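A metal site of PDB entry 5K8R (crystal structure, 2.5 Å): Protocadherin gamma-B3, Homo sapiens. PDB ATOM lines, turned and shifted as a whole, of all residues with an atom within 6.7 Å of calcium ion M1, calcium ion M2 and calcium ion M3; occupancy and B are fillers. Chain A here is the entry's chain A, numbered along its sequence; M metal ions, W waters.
The side-chain amide nitrogen (ND2) of Asn 313 lies close to the side-chain carboxylate (OD1) of Asp 312 (3.0 Å).
OE1 of Glu 223 lies close to N of Phe 279, at 2.8 Å.
The backbone NH (N) of Glu 223 sits at hydrogen-bond distance from the backbone carbonyl oxygen (O) of Ser 308 (3.4 Å).
ND2 of Asn 349 sits at hydrogen-bond distance from OD2 of Asp 309 (3.1 Å).
OD2 of Asp 309 lies within hydrogen-bond range of N of Ser 346.
N of Leu 402 lies within hydrogen-bond range of OD1 of Asp 396.
Within 4 Å of calcium ion M1: Glu 223, Glu 280, Asp 309, Glu 310, Asp 312, Asn 313 and Asp 345.
Along chain A the residues within 4 Å of calcium ion M1 span positions 223 to 345.
The nearest printed residue that does not touch calcium ion M1 is Phe 279 (4.6 Å).
Within 4 Å of calcium ion M2: Asn 311, Asn 313, Asp 343, Asp 345, Asn 349 and Asp 396.
Within 4 Å of calcium ion M3: Glu 223, Asp 278, Glu 280, Asp 312 and Asn 313.
Calcium ion M1 is bound by the backbone carbonyl oxygen (O) of Glu 310 (2.4 Å), the side-chain carboxylate (OE2) of Glu 223 (2.5 Å), the side-chain carboxylate (OD1) of Asp 309 (2.5 Å), the side-chain carboxylate (OE2) of Glu 280 (2.5 Å), the side-chain carboxylate (OD1) of Asp 345 (2.5 Å), the side-chain carboxylate (OD1) of Asp 312 (2.7 Å) and the side-chain carboxylate (OE1) of Glu 280 (2.7 Å).
Calcium ion M2 is bound by O of Asn 313 (2.4 Å), OD1 of Asp 343 (2.5 Å), OD1 of Asn 311 (2.5 Å), O of Asn 349 (2.5 Å), OD2 of Asp 345 (2.5 Å), OD2 of Asp 343 (2.6 Å) and OD2 of Asp 396 (2.7 Å).
Calcium ion M2 has seven donor atoms within binding distance.
Calcium ion M3 is bound by OE1 of Glu 280 (2.4 Å), OD2 of Asp 312 (2.4 Å), OE1 of Glu 223 (2.5 Å), OD1 of Asp 278 (2.5 Å) and water W1 (2.5 Å).
Calcium ion M3 has five donor atoms within binding distance.
Slightly farther from calcium ion M3 lies the side-chain carboxylate (OD1) of Asp 312 (2.9 Å).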
ATOM      1  N   GLU A 223     -15.744   1.340  14.254  1.00  0.00           N
ATOM      2  CA  GLU A 223     -16.847   0.392  14.391  1.00  0.00           C
ATOM      3  C   GLU A 223     -17.052  -0.422  13.118  1.00  0.00           C
ATOM      4  O   GLU A 223     -17.560  -1.547  13.183  1.00  0.00           O
ATOM      5  CB  GLU A 223     -18.136   1.118  14.767  1.00  0.00           C
ATOM      6  CG  GLU A 223     -18.503   2.251  13.835  1.00  0.00           C
ATOM      7  CD  GLU A 223     -19.875   2.829  14.134  1.00  0.00           C
ATOM      8  OE1 GLU A 223     -20.707   2.097  14.714  1.00  0.00           O
ATOM      9  OE2 GLU A 223     -20.115   4.010  13.808  1.00  0.00           O
ATOM     10  N   LEU A 277     -18.519  -4.785  15.351  1.00  0.00           N
ATOM     11  CA  LEU A 277     -18.511  -3.703  16.321  1.00  0.00           C
ATOM     12  C   LEU A 277     -19.554  -2.666  15.944  1.00  0.00           C
ATOM     13  O   LEU A 277     -19.732  -2.337  14.765  1.00  0.00           O
ATOM     14  CB  LEU A 277     -17.133  -3.058  16.400  1.00  0.00           C
ATOM     15  CG  LEU A 277     -15.953  -3.869  16.963  1.00  0.00           C
ATOM     16  CD1 LEU A 277     -16.404  -4.726  18.139  1.00  0.00           C
ATOM     17  CD2 LEU A 277     -15.313  -4.730  15.882  1.00  0.00           C
ATOM     18  N   ASP A 278     -20.247  -2.140  16.950  1.00  0.00           N
ATOM     19  CA  ASP A 278     -21.278  -1.124  16.744  1.00  0.00           C
ATOM     20  C   ASP A 278     -21.100  -0.040  17.796  1.00  0.00           C
ATOM     21  O   ASP A 278     -21.363  -0.269  18.980  1.00  0.00           O
ATOM     22  CB  ASP A 278     -22.677  -1.732  16.810  1.00  0.00           C
ATOM     23  CG  ASP A 278     -23.757  -0.760  16.371  1.00  0.00           C
ATOM     24  OD1 ASP A 278     -23.425   0.224  15.667  1.00  0.00           O
ATOM     25  OD2 ASP A 278     -24.930  -0.970  16.723  1.00  0.00           O
ATOM     26  N   PHE A 279     -20.639   1.135  17.356  1.00  0.00           N
ATOM     27  CA  PHE A 279     -20.447   2.253  18.285  1.00  0.00           C
ATOM     28  C   PHE A 279     -21.763   2.656  18.943  1.00  0.00           C
ATOM     29  O   PHE A 279     -21.766   3.086  20.104  1.00  0.00           O
ATOM     30  CB  PHE A 279     -19.839   3.440  17.547  1.00  0.00           C
ATOM     31  CG  PHE A 279     -19.626   4.656  18.407  1.00  0.00           C
ATOM     32  CD1 PHE A 279     -18.474   4.792  19.157  1.00  0.00           C
ATOM     33  CD2 PHE A 279     -20.584   5.658  18.459  1.00  0.00           C
ATOM     34  CE1 PHE A 279     -18.274   5.911  19.945  1.00  0.00           C
ATOM     35  CE2 PHE A 279     -20.394   6.778  19.248  1.00  0.00           C
ATOM     36  CZ  PHE A 279     -19.232   6.905  20.002  1.00  0.00           C
ATOM     37  N   GLU A 280     -22.882   2.516  18.235  1.00  0.00           N
ATOM     38  CA  GLU A 280     -24.174   2.874  18.797  1.00  0.00           C
ATOM     39  C   GLU A 280     -24.588   1.955  19.930  1.00  0.00           C
ATOM     40  O   GLU A 280     -25.421   2.350  20.757  1.00  0.00           O
ATOM     41  CB  GLU A 280     -25.244   2.872  17.707  1.00  0.00           C
ATOM     42  CG  GLU A 280     -25.320   4.154  16.895  1.00  0.00           C
ATOM     43  CD  GLU A 280     -24.065   4.431  16.102  1.00  0.00           C
ATOM     44  OE1 GLU A 280     -23.528   3.485  15.487  1.00  0.00           O
ATOM     45  OE2 GLU A 280     -23.607   5.594  16.094  1.00  0.00           O
ATOM     46  N   GLU A 281     -24.029   0.747  20.005  1.00  0.00           N
ATOM     47  CA  GLU A 281     -24.369  -0.184  21.073  1.00  0.00           C
ATOM     48  C   GLU A 281     -23.408  -0.087  22.247  1.00  0.00           C
ATOM     49  O   GLU A 281     -23.836  -0.006  23.398  1.00  0.00           O
ATOM     50  CB  GLU A 281     -24.405  -1.613  20.525  1.00  0.00           C
ATOM     51  CG  GLU A 281     -24.871  -2.653  21.536  1.00  0.00           C
ATOM     52  CD  GLU A 281     -26.314  -2.452  21.970  1.00  0.00           C
ATOM     53  OE1 GLU A 281     -27.117  -1.927  21.157  1.00  0.00           O
ATOM     54  OE2 GLU A 281     -26.651  -2.799  23.115  1.00  0.00           O
ATOM     55  N   SER A 308     -14.462   3.981  17.890  1.00  0.00           N
ATOM     56  CA  SER A 308     -14.702   5.322  17.397  1.00  0.00           C
ATOM     57  C   SER A 308     -15.913   5.351  16.478  1.00  0.00           C
ATOM     58  O   SER A 308     -16.235   4.357  15.806  1.00  0.00           O
ATOM     59  CB  SER A 308     -13.470   5.859  16.653  1.00  0.00           C
ATOM     60  OG  SER A 308     -13.065   4.958  15.637  1.00  0.00           O
ATOM     61  N   ASP A 309     -16.589   6.499  16.457  1.00  0.00           N
ATOM     62  CA  ASP A 309     -17.858   6.623  15.738  1.00  0.00           C
ATOM     63  C   ASP A 309     -17.628   6.771  14.237  1.00  0.00           C
ATOM     64  O   ASP A 309     -16.715   7.483  13.802  1.00  0.00           O
ATOM     65  CB  ASP A 309     -18.646   7.819  16.276  1.00  0.00           C
ATOM     66  CG  ASP A 309     -19.987   7.979  15.585  1.00  0.00           C
ATOM     67  OD1 ASP A 309     -20.608   6.958  15.236  1.00  0.00           O
ATOM     68  OD2 ASP A 309     -20.421   9.143  15.396  1.00  0.00           O
ATOM     69  N   GLU A 310     -18.467   6.088  13.458  1.00  0.00           N
ATOM     70  CA  GLU A 310     -18.480   6.215  12.013  1.00  0.00           C
ATOM     71  C   GLU A 310     -19.881   6.618  11.559  1.00  0.00           C
ATOM     72  O   GLU A 310     -20.880   6.302  12.212  1.00  0.00           O
ATOM     73  CB  GLU A 310     -18.082   4.899  11.324  1.00  0.00           C
ATOM     74  CG  GLU A 310     -16.589   4.612  11.365  1.00  0.00           C
ATOM     75  CD  GLU A 310     -15.819   5.411  10.334  1.00  0.00           C
ATOM     76  OE1 GLU A 310     -16.218   5.395   9.151  1.00  0.00           O
ATOM     77  OE2 GLU A 310     -14.821   6.063  10.698  1.00  0.00           O
ATOM     78  N   ASN A 311     -19.938   7.334  10.438  1.00  0.00           N
ATOM     79  CA  ASN A 311     -21.213   7.849   9.924  1.00  0.00           C
ATOM     80  C   ASN A 311     -21.890   6.774   9.074  1.00  0.00           C
ATOM     81  O   ASN A 311     -21.936   6.829   7.845  1.00  0.00           O
ATOM     82  CB  ASN A 311     -20.983   9.127   9.127  1.00  0.00           C
ATOM     83  CG  ASN A 311     -22.279   9.841   8.798  1.00  0.00           C
ATOM     84  OD1 ASN A 311     -23.293   9.669   9.479  1.00  0.00           O
ATOM     85  ND2 ASN A 311     -22.251  10.659   7.755  1.00  0.00           N
ATOM     86  N   ASP A 312     -22.422   5.762   9.772  1.00  0.00           N
ATOM     87  CA  ASP A 312     -23.087   4.640   9.129  1.00  0.00           C
ATOM     88  C   ASP A 312     -24.576   4.583   9.422  1.00  0.00           C
ATOM     89  O   ASP A 312     -25.201   3.532   9.308  1.00  0.00           O
ATOM     90  CB  ASP A 312     -22.424   3.321   9.543  1.00  0.00           C
ATOM     91  CG  ASP A 312     -22.600   3.018  11.026  1.00  0.00           C
ATOM     92  OD1 ASP A 312     -22.722   3.972  11.823  1.00  0.00           O
ATOM     93  OD2 ASP A 312     -22.613   1.825  11.381  1.00  0.00           O
ATOM     94  N   ASN A 313     -25.175   5.718   9.808  1.00  0.00           N
ATOM     95  CA  ASN A 313     -26.602   5.812  10.054  1.00  0.00           C
ATOM     96  C   ASN A 313     -27.139   7.062   9.378  1.00  0.00           C
ATOM     97  O   ASN A 313     -26.692   8.168   9.679  1.00  0.00           O
ATOM     98  CB  ASN A 313     -26.903   5.848  11.562  1.00  0.00           C
ATOM     99  CG  ASN A 313     -26.753   4.484  12.221  1.00  0.00           C
ATOM    100  OD1 ASN A 313     -27.725   3.731  12.321  1.00  0.00           O
ATOM    101  ND2 ASN A 313     -25.550   4.181  12.668  1.00  0.00           N
ATOM    102  N   ALA A 314     -28.091   6.872   8.471  1.00  0.00           N
ATOM    103  CA  ALA A 314     -28.677   7.982   7.741  1.00  0.00           C
ATOM    104  C   ALA A 314     -29.694   8.726   8.597  1.00  0.00           C
ATOM    105  O   ALA A 314     -30.333   8.126   9.474  1.00  0.00           O
ATOM    106  CB  ALA A 314     -29.347   7.493   6.459  1.00  0.00           C
ATOM    107  N   PRO A 315     -29.850  10.035   8.395  1.00  0.00           N
ATOM    108  CA  PRO A 315     -30.854  10.787   9.164  1.00  0.00           C
ATOM    109  C   PRO A 315     -32.258  10.282   8.877  1.00  0.00           C
ATOM    110  O   PRO A 315     -32.555   9.795   7.779  1.00  0.00           O
ATOM    111  CB  PRO A 315     -30.668  12.231   8.677  1.00  0.00           C
ATOM    112  CG  PRO A 315     -29.279  12.266   8.116  1.00  0.00           C
ATOM    113  CD  PRO A 315     -29.051  10.914   7.535  1.00  0.00           C
ATOM    114  N   ASP A 343     -30.862  11.270  14.276  1.00  0.00           N
ATOM    115  CA  ASP A 343     -29.735  10.526  13.732  1.00  0.00           C
ATOM    116  C   ASP A 343     -29.062   9.770  14.866  1.00  0.00           C
ATOM    117  O   ASP A 343     -28.775  10.347  15.918  1.00  0.00           O
ATOM    118  CB  ASP A 343     -28.739  11.453  13.040  1.00  0.00           C
ATOM    119  CG  ASP A 343     -27.777  10.715  12.122  1.00  0.00           C
ATOM    120  OD1 ASP A 343     -27.625  11.127  10.953  1.00  0.00           O
ATOM    121  OD2 ASP A 343     -27.181   9.708  12.564  1.00  0.00           O
ATOM    122  N   LEU A 344     -28.809   8.480  14.649  1.00  0.00           N
ATOM    123  CA  LEU A 344     -28.261   7.636  15.703  1.00  0.00           C
ATOM    124  C   LEU A 344     -26.782   7.874  15.959  1.00  0.00           C
ATOM    125  O   LEU A 344     -26.271   7.471  17.013  1.00  0.00           O
ATOM    126  CB  LEU A 344     -28.488   6.161  15.364  1.00  0.00           C
ATOM    127  CG  LEU A 344     -29.935   5.708  15.184  1.00  0.00           C
ATOM    128  CD1 LEU A 344     -30.003   4.233  14.815  1.00  0.00           C
ATOM    129  CD2 LEU A 344     -30.759   5.986  16.439  1.00  0.00           C
ATOM    130  N   ASP A 345     -26.078   8.520  15.035  1.00  0.00           N
ATOM    131  CA  ASP A 345     -24.645   8.733  15.174  1.00  0.00           C
ATOM    132  C   ASP A 345     -24.371   9.880  16.152  1.00  0.00           C
ATOM    133  O   ASP A 345     -25.283  10.545  16.641  1.00  0.00           O
ATOM    134  CB  ASP A 345     -24.006   8.993  13.813  1.00  0.00           C
ATOM    135  CG  ASP A 345     -24.158   7.828  12.869  1.00  0.00           C
ATOM    136  OD1 ASP A 345     -24.184   6.670  13.346  1.00  0.00           O
ATOM    137  OD2 ASP A 345     -24.256   8.051  11.640  1.00  0.00           O
ATOM    138  N   SER A 346     -23.094  10.111  16.437  1.00  0.00           N
ATOM    139  CA  SER A 346     -22.672  11.125  17.391  1.00  0.00           C
ATOM    140  C   SER A 346     -21.856  12.202  16.685  1.00  0.00           C
ATOM    141  O   SER A 346     -21.400  12.027  15.557  1.00  0.00           O
ATOM    142  CB  SER A 346     -21.846  10.497  18.519  1.00  0.00           C
ATOM    143  OG  SER A 346     -22.544   9.442  19.145  1.00  0.00           O
ATOM    144  N   PHE A 348     -20.746  15.519  14.689  1.00  0.00           N
ATOM    145  CA  PHE A 348     -21.250  16.066  13.441  1.00  0.00           C
ATOM    146  C   PHE A 348     -21.879  14.990  12.560  1.00  0.00           C
ATOM    147  O   PHE A 348     -22.661  15.326  11.661  1.00  0.00           O
ATOM    148  CB  PHE A 348     -20.133  16.779  12.681  1.00  0.00           C
ATOM    149  CG  PHE A 348     -19.842  18.166  13.205  1.00  0.00           C
ATOM    150  CD1 PHE A 348     -20.708  19.212  12.963  1.00  0.00           C
ATOM    151  CD2 PHE A 348     -18.693  18.411  13.943  1.00  0.00           C
ATOM    152  CE1 PHE A 348     -20.450  20.485  13.440  1.00  0.00           C
ATOM    153  CE2 PHE A 348     -18.425  19.678  14.432  1.00  0.00           C
ATOM    154  CZ  PHE A 348     -19.304  20.717  14.174  1.00  0.00           C
ATOM    155  N   ASN A 349     -21.561  13.715  12.795  1.00  0.00           N
ATOM    156  CA  ASN A 349     -22.272  12.648  12.118  1.00  0.00           C
ATOM    157  C   ASN A 349     -23.740  12.593  12.522  1.00  0.00           C
ATOM    158  O   ASN A 349     -24.555  12.025  11.792  1.00  0.00           O
ATOM    159  CB  ASN A 349     -21.605  11.296  12.411  1.00  0.00           C
ATOM    160  CG  ASN A 349     -20.132  11.281  12.068  1.00  0.00           C
ATOM    161  OD1 ASN A 349     -19.691  11.909  11.098  1.00  0.00           O
ATOM    162  ND2 ASN A 349     -19.341  10.567  12.870  1.00  0.00           N
ATOM    163  N   GLY A 350     -24.083  13.181  13.671  1.00  0.00           N
ATOM    164  CA  GLY A 350     -25.454  13.186  14.139  1.00  0.00           C
ATOM    165  C   GLY A 350     -26.155  14.512  13.959  1.00  0.00           C
ATOM    166  O   GLY A 350     -27.383  14.586  14.087  1.00  0.00           O
ATOM    167  N   GLU A 351     -25.406  15.569  13.656  1.00  0.00           N
ATOM    168  CA  GLU A 351     -26.014  16.852  13.355  1.00  0.00           C
ATOM    169  C   GLU A 351     -26.783  16.763  12.049  1.00  0.00           C
ATOM    170  O   GLU A 351     -26.339  16.122  11.093  1.00  0.00           O
ATOM    171  CB  GLU A 351     -24.943  17.948  13.271  1.00  0.00           C
ATOM    172  CG  GLU A 351     -24.106  18.104  14.528  1.00  0.00           C
ATOM    173  CD  GLU A 351     -24.907  18.615  15.711  1.00  0.00           C
ATOM    174  OE1 GLU A 351     -25.949  19.269  15.494  1.00  0.00           O
ATOM    175  OE2 GLU A 351     -24.495  18.360  16.865  1.00  0.00           O
ATOM    176  N   ASP A 396     -27.009  14.721   7.104  1.00  0.00           N
ATOM    177  CA  ASP A 396     -26.127  14.910   8.243  1.00  0.00           C
ATOM    178  C   ASP A 396     -24.855  15.631   7.818  1.00  0.00           C
ATOM    179  O   ASP A 396     -24.650  15.939   6.638  1.00  0.00           O
ATOM    180  CB  ASP A 396     -25.819  13.571   8.918  1.00  0.00           C
ATOM    181  CG  ASP A 396     -25.269  12.539   7.945  1.00  0.00           C
ATOM    182  OD1 ASP A 396     -24.671  12.912   6.922  1.00  0.00           O
ATOM    183  OD2 ASP A 396     -25.436  11.326   8.213  1.00  0.00           O
ATOM    184  N   LYS A 397     -23.984  15.910   8.785  1.00  0.00           N
ATOM    185  CA  LYS A 397     -22.738  16.621   8.542  1.00  0.00           C
ATOM    186  C   LYS A 397     -21.520  15.718   8.699  1.00  0.00           C
ATOM    187  O   LYS A 397     -20.449  16.161   9.115  1.00  0.00           O
ATOM    188  CB  LYS A 397     -22.621  17.824   9.484  1.00  0.00           C
ATOM    189  CG  LYS A 397     -23.845  18.743   9.457  1.00  0.00           C
ATOM    190  CD  LYS A 397     -23.620  19.974  10.306  1.00  0.00           C
ATOM    191  CE  LYS A 397     -24.908  20.785  10.442  1.00  0.00           C
ATOM    192  NZ  LYS A 397     -25.480  21.149   9.121  1.00  0.00           N
ATOM    193  N   GLY A 398     -21.666  14.433   8.347  1.00  0.00           N
ATOM    194  CA  GLY A 398     -20.573  13.492   8.432  1.00  0.00           C
ATOM    195  C   GLY A 398     -19.730  13.461   7.168  1.00  0.00           C
ATOM    196  O   GLY A 398     -19.989  14.166   6.192  1.00  0.00           O
ATOM    197  N   LEU A 402     -24.549  11.561   4.773  1.00  0.00           N
ATOM    198  CA  LEU A 402     -25.680  10.722   4.419  1.00  0.00           C
ATOM    199  C   LEU A 402     -26.962  11.533   4.496  1.00  0.00           C
ATOM    200  O   LEU A 402     -27.044  12.519   5.235  1.00  0.00           O
ATOM    201  CB  LEU A 402     -25.790   9.484   5.334  1.00  0.00           C
ATOM    202  CG  LEU A 402     -24.903   8.277   5.003  1.00  0.00           C
ATOM    203  CD1 LEU A 402     -23.433   8.555   5.308  1.00  0.00           C
ATOM    204  CD2 LEU A 402     -25.373   7.050   5.760  1.00  0.00           C
HETATM  205 CA    CA M   1     -22.141   5.377  14.090  1.00  0.00          CA
HETATM  206 CA    CA M   2     -25.445  10.048  10.602  1.00  0.00          CA
HETATM  207 CA    CA M   3     -22.986   1.832  13.792  1.00  0.00          CA
HETATM  208  O   HOH W   1     -22.701  -0.656  13.454  1.00  0.00           O
HETATM  209  O   HOH W   2     -25.772   1.136  11.826  1.00  0.00           O
